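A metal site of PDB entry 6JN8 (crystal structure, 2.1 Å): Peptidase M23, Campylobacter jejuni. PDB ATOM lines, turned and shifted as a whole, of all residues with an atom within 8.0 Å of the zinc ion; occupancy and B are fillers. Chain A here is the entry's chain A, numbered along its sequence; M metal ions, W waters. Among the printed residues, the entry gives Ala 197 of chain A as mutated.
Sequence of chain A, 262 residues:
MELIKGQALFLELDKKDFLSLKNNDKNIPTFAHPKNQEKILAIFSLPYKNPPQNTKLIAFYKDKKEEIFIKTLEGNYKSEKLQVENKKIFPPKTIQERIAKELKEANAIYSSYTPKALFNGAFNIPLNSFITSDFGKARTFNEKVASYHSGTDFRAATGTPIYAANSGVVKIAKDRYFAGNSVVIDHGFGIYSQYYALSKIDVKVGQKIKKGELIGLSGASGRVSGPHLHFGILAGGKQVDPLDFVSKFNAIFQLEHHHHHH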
ATOM      1  N   THR A 132       2.193 -23.081  17.392  1.00  0.00           N
ATOM      2  CA  THR A 132       1.022 -22.568  18.084  1.00  0.00           C
ATOM      3  C   THR A 132       1.359 -21.384  18.984  1.00  0.00           C
ATOM      4  O   THR A 132       0.510 -20.526  19.206  1.00  0.00           O
ATOM      5  CB  THR A 132       0.355 -23.659  18.931  1.00  0.00           C
ATOM      6  OG1 THR A 132       1.331 -24.252  19.800  1.00  0.00           O
ATOM      7  CG2 THR A 132      -0.230 -24.725  18.036  1.00  0.00           C
ATOM      8  N   SER A 133       2.584 -21.332  19.500  1.00  0.00           N
ATOM      9  CA  SER A 133       3.021 -20.228  20.346  1.00  0.00           C
ATOM     10  C   SER A 133       4.510 -20.049  20.097  1.00  0.00           C
ATOM     11  O   SER A 133       5.291 -20.957  20.390  1.00  0.00           O
ATOM     12  CB  SER A 133       2.725 -20.534  21.812  1.00  0.00           C
ATOM     13  OG  SER A 133       3.108 -19.469  22.652  1.00  0.00           O
ATOM     14  N   ASP A 134       4.914 -18.906  19.541  1.00  0.00           N
ATOM     15  CA  ASP A 134       6.288 -18.768  19.104  1.00  0.00           C
ATOM     16  C   ASP A 134       7.188 -18.252  20.233  1.00  0.00           C
ATOM     17  O   ASP A 134       6.744 -17.874  21.319  1.00  0.00           O
ATOM     18  CB  ASP A 134       6.395 -17.861  17.872  1.00  0.00           C
ATOM     19  CG  ASP A 134       7.572 -18.242  16.927  1.00  0.00           C
ATOM     20  OD1 ASP A 134       8.396 -19.147  17.254  1.00  0.00           O
ATOM     21  OD2 ASP A 134       7.677 -17.619  15.836  1.00  0.00           O
ATOM     22  N   PHE A 135       8.498 -18.279  19.948  1.00  0.00           N
ATOM     23  CA  PHE A 135       9.541 -17.833  20.875  1.00  0.00           C
ATOM     24  C   PHE A 135       9.334 -16.379  21.282  1.00  0.00           C
ATOM     25  O   PHE A 135       8.880 -15.536  20.509  1.00  0.00           O
ATOM     26  CB  PHE A 135      10.901 -18.001  20.204  1.00  0.00           C
ATOM     27  CG  PHE A 135      12.071 -17.509  21.017  1.00  0.00           C
ATOM     28  CD1 PHE A 135      12.711 -18.347  21.921  1.00  0.00           C
ATOM     29  CD2 PHE A 135      12.553 -16.215  20.845  1.00  0.00           C
ATOM     30  CE1 PHE A 135      13.816 -17.891  22.657  1.00  0.00           C
ATOM     31  CE2 PHE A 135      13.647 -15.751  21.584  1.00  0.00           C
ATOM     32  CZ  PHE A 135      14.281 -16.597  22.489  1.00  0.00           C
ATOM     33  N   HIS A 149       8.831 -16.834  26.775  1.00  0.00           N
ATOM     34  CA  HIS A 149       8.851 -18.178  26.205  1.00  0.00           C
ATOM     35  C   HIS A 149      10.209 -18.439  25.550  1.00  0.00           C
ATOM     36  O   HIS A 149      10.547 -17.817  24.543  1.00  0.00           O
ATOM     37  CB  HIS A 149       7.705 -18.317  25.197  1.00  0.00           C
ATOM     38  CG  HIS A 149       7.389 -19.733  24.815  1.00  0.00           C
ATOM     39  ND1 HIS A 149       6.786 -20.062  23.614  1.00  0.00           N
ATOM     40  CD2 HIS A 149       7.597 -20.894  25.469  1.00  0.00           C
ATOM     41  CE1 HIS A 149       6.640 -21.368  23.547  1.00  0.00           C
ATOM     42  NE2 HIS A 149       7.121 -21.901  24.660  1.00  0.00           N
ATOM     43  N   SER A 150      10.995 -19.358  26.120  1.00  0.00           N
ATOM     44  CA  SER A 150      12.378 -19.555  25.695  1.00  0.00           C
ATOM     45  C   SER A 150      12.522 -20.649  24.623  1.00  0.00           C
ATOM     46  O   SER A 150      13.622 -21.146  24.406  1.00  0.00           O
ATOM     47  CB  SER A 150      13.269 -19.859  26.910  1.00  0.00           C
ATOM     48  OG  SER A 150      12.884 -21.075  27.518  1.00  0.00           O
ATOM     49  N   GLY A 151      11.422 -21.024  23.981  1.00  0.00           N
ATOM     50  CA  GLY A 151      11.413 -21.941  22.865  1.00  0.00           C
ATOM     51  C   GLY A 151      10.157 -21.709  22.062  1.00  0.00           C
ATOM     52  O   GLY A 151       9.428 -20.733  22.290  1.00  0.00           O
ATOM     53  N   THR A 152       9.876 -22.608  21.125  1.00  0.00           N
ATOM     54  CA  THR A 152       8.708 -22.485  20.268  1.00  0.00           C
ATOM     55  C   THR A 152       7.859 -23.746  20.370  1.00  0.00           C
ATOM     56  O   THR A 152       8.391 -24.855  20.513  1.00  0.00           O
ATOM     57  CB  THR A 152       9.111 -22.201  18.808  1.00  0.00           C
ATOM     58  OG1 THR A 152       7.953 -21.841  18.044  1.00  0.00           O
ATOM     59  CG2 THR A 152       9.777 -23.408  18.162  1.00  0.00           C
ATOM     60  N   ASP A 153       6.529 -23.591  20.313  1.00  0.00           N
ATOM     61  CA  ASP A 153       5.596 -24.692  20.531  1.00  0.00           C
ATOM     62  C   ASP A 153       4.948 -25.129  19.219  1.00  0.00           C
ATOM     63  O   ASP A 153       4.410 -24.291  18.495  1.00  0.00           O
ATOM     64  CB  ASP A 153       4.511 -24.296  21.540  1.00  0.00           C
ATOM     65  CG  ASP A 153       5.027 -24.294  22.978  1.00  0.00           C
ATOM     66  OD1 ASP A 153       6.134 -24.826  23.193  1.00  0.00           O
ATOM     67  OD2 ASP A 153       4.329 -23.757  23.863  1.00  0.00           O
ATOM     68  N   PHE A 154       4.979 -26.432  18.950  1.00  0.00           N
ATOM     69  CA  PHE A 154       4.309 -27.024  17.794  1.00  0.00           C
ATOM     70  C   PHE A 154       3.048 -27.753  18.233  1.00  0.00           C
ATOM     71  O   PHE A 154       3.063 -28.480  19.231  1.00  0.00           O
ATOM     72  CB  PHE A 154       5.202 -28.043  17.079  1.00  0.00           C
ATOM     73  CG  PHE A 154       6.371 -27.464  16.376  1.00  0.00           C
ATOM     74  CD1 PHE A 154       7.504 -27.059  17.081  1.00  0.00           C
ATOM     75  CD2 PHE A 154       6.365 -27.365  14.991  1.00  0.00           C
ATOM     76  CE1 PHE A 154       8.605 -26.559  16.415  1.00  0.00           C
ATOM     77  CE2 PHE A 154       7.442 -26.862  14.324  1.00  0.00           C
ATOM     78  CZ  PHE A 154       8.566 -26.467  15.017  1.00  0.00           C
ATOM     79  N   TYR A 196      10.968 -30.792  24.765  1.00  0.00           N
ATOM     80  CA  TYR A 196      10.434 -30.804  26.124  1.00  0.00           C
ATOM     81  C   TYR A 196       8.978 -31.223  26.137  1.00  0.00           C
ATOM     82  O   TYR A 196       8.285 -31.191  25.110  1.00  0.00           O
ATOM     83  CB  TYR A 196      10.576 -29.433  26.798  1.00  0.00           C
ATOM     84  CG  TYR A 196      11.984 -28.964  27.061  1.00  0.00           C
ATOM     85  CD1 TYR A 196      13.072 -29.815  26.869  1.00  0.00           C
ATOM     86  CD2 TYR A 196      12.234 -27.663  27.490  1.00  0.00           C
ATOM     87  CE1 TYR A 196      14.368 -29.387  27.111  1.00  0.00           C
ATOM     88  CE2 TYR A 196      13.536 -27.227  27.730  1.00  0.00           C
ATOM     89  CZ  TYR A 196      14.593 -28.096  27.532  1.00  0.00           C
ATOM     90  OH  TYR A 196      15.884 -27.676  27.776  1.00  0.00           O
ATOM     91  N   ALA A 197       8.523 -31.612  27.327  1.00  0.00           N
ATOM     92  CA  ALA A 197       7.126 -31.954  27.619  1.00  0.00           C
ATOM     93  C   ALA A 197       6.717 -33.257  26.944  1.00  0.00           C
ATOM     94  O   ALA A 197       5.537 -33.477  26.664  1.00  0.00           O
ATOM     95  CB  ALA A 197       6.181 -30.817  27.207  1.00  0.00           C
ATOM     96  N   ARG A 223      -0.950 -29.661  30.495  1.00  0.00           N
ATOM     97  CA  ARG A 223      -0.173 -28.439  30.698  1.00  0.00           C
ATOM     98  C   ARG A 223      -1.128 -27.269  30.744  1.00  0.00           C
ATOM     99  O   ARG A 223      -2.328 -27.392  30.461  1.00  0.00           O
ATOM    100  CB  ARG A 223       0.866 -28.238  29.590  1.00  0.00           C
ATOM    101  CG  ARG A 223       2.132 -29.019  29.832  1.00  0.00           C
ATOM    102  CD  ARG A 223       3.194 -28.222  30.535  1.00  0.00           C
ATOM    103  NE  ARG A 223       4.373 -29.053  30.684  1.00  0.00           N
ATOM    104  CZ  ARG A 223       5.437 -28.741  31.420  1.00  0.00           C
ATOM    105  NH1 ARG A 223       5.466 -27.600  32.097  1.00  0.00           N
ATOM    106  NH2 ARG A 223       6.464 -29.590  31.476  1.00  0.00           N
ATOM    107  N   SER A 225      -1.606 -25.155  28.710  1.00  0.00           N
ATOM    108  CA  SER A 225      -2.173 -24.898  27.386  1.00  0.00           C
ATOM    109  C   SER A 225      -2.390 -26.161  26.545  1.00  0.00           C
ATOM    110  O   SER A 225      -2.701 -26.046  25.348  1.00  0.00           O
ATOM    111  CB  SER A 225      -1.270 -23.936  26.611  1.00  0.00           C
ATOM    112  OG  SER A 225      -0.003 -24.532  26.349  1.00  0.00           O
ATOM    113  N   HIS A 228       1.384 -30.418  23.106  1.00  0.00           N
ATOM    114  CA  HIS A 228       2.237 -29.725  22.147  1.00  0.00           C
ATOM    115  C   HIS A 228       3.655 -30.223  22.351  1.00  0.00           C
ATOM    116  O   HIS A 228       3.965 -30.849  23.365  1.00  0.00           O
ATOM    117  CB  HIS A 228       2.192 -28.200  22.328  1.00  0.00           C
ATOM    118  CG  HIS A 228       2.689 -27.732  23.659  1.00  0.00           C
ATOM    119  ND1 HIS A 228       1.869 -27.626  24.761  1.00  0.00           N
ATOM    120  CD2 HIS A 228       3.932 -27.385  24.073  1.00  0.00           C
ATOM    121  CE1 HIS A 228       2.577 -27.211  25.799  1.00  0.00           C
ATOM    122  NE2 HIS A 228       3.837 -27.059  25.409  1.00  0.00           N
ATOM    123  N   LEU A 229       4.519 -29.963  21.360  1.00  0.00           N
ATOM    124  CA  LEU A 229       5.962 -30.120  21.514  1.00  0.00           C
ATOM    125  C   LEU A 229       6.574 -28.749  21.721  1.00  0.00           C
ATOM    126  O   LEU A 229       6.300 -27.828  20.957  1.00  0.00           O
ATOM    127  CB  LEU A 229       6.584 -30.802  20.281  1.00  0.00           C
ATOM    128  CG  LEU A 229       8.081 -31.142  20.088  1.00  0.00           C
ATOM    129  CD1 LEU A 229       8.885 -29.994  19.496  1.00  0.00           C
ATOM    130  CD2 LEU A 229       8.775 -31.720  21.351  1.00  0.00           C
ATOM    131  N   HIS A 230       7.364 -28.605  22.784  1.00  0.00           N
ATOM    132  CA  HIS A 230       8.173 -27.408  22.966  1.00  0.00           C
ATOM    133  C   HIS A 230       9.564 -27.706  22.401  1.00  0.00           C
ATOM    134  O   HIS A 230      10.220 -28.678  22.795  1.00  0.00           O
ATOM    135  CB  HIS A 230       8.243 -27.009  24.447  1.00  0.00           C
ATOM    136  CG  HIS A 230       9.344 -26.038  24.762  1.00  0.00           C
ATOM    137  ND1 HIS A 230       9.087 -24.732  25.128  1.00  0.00           N
ATOM    138  CD2 HIS A 230      10.691 -26.175  24.791  1.00  0.00           C
ATOM    139  CE1 HIS A 230      10.234 -24.106  25.366  1.00  0.00           C
ATOM    140  NE2 HIS A 230      11.222 -24.969  25.155  1.00  0.00           N
ATOM    141  N   PHE A 231       9.998 -26.871  21.470  1.00  0.00           N
ATOM    142  CA  PHE A 231      11.258 -27.026  20.778  1.00  0.00           C
ATOM    143  C   PHE A 231      12.140 -25.839  21.119  1.00  0.00           C
ATOM    144  O   PHE A 231      11.700 -24.691  21.039  1.00  0.00           O
ATOM    145  CB  PHE A 231      11.032 -27.094  19.263  1.00  0.00           C
ATOM    146  CG  PHE A 231      12.285 -27.270  18.465  1.00  0.00           C
ATOM    147  CD1 PHE A 231      13.042 -28.420  18.609  1.00  0.00           C
ATOM    148  CD2 PHE A 231      12.711 -26.296  17.576  1.00  0.00           C
ATOM    149  CE1 PHE A 231      14.203 -28.605  17.871  1.00  0.00           C
ATOM    150  CE2 PHE A 231      13.862 -26.466  16.823  1.00  0.00           C
ATOM    151  CZ  PHE A 231      14.610 -27.620  16.977  1.00  0.00           C
ATOM    152  N   GLY A 232      13.389 -26.117  21.512  1.00  0.00           N
ATOM    153  CA  GLY A 232      14.307 -25.058  21.884  1.00  0.00           C
ATOM    154  C   GLY A 232      15.644 -25.228  21.190  1.00  0.00           C
ATOM    155  O   GLY A 232      16.016 -26.321  20.757  1.00  0.00           O
HETATM  156 ZN    ZN M   1       6.935 -23.898  25.185  1.00  0.00          ZN
HETATM  157  O   HOH W   1       5.954 -24.836  27.114  1.00  0.00           O
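O of Gly 151 is in hydrogen-bond range of ND1 of His 149, at 3.0 Å.
ND1 of His 149 sits at hydrogen-bond distance from O of Asp 134, at 3.2 Å.
O of His 230 is in hydrogen-bond range of N of Tyr 196 (3.0 Å).
N of Asp 153 is in hydrogen-bond range of O of Ser 133.
The backbone NH of Thr 132 sits at hydrogen-bond distance from the backbone carbonyl oxygen of Asp 153, 2.8 Å away.
Three residues have an atom within 4 Å of the zinc ion: His 149, Asp 153 and His 230.
The nearest printed residue that does not touch the zinc ion is His 228 (4.4 Å).
NE2 of His 149 binds the zinc ion (2.1 Å).
The zinc ion is bound by ND1 of His 230, at 2.3 Å.
The zinc ion is bound by OD1 of Asp 153, at 2.3 Å.
Water W1 is bound to the zinc ion.
The zinc ion has four donor atoms within binding distance.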
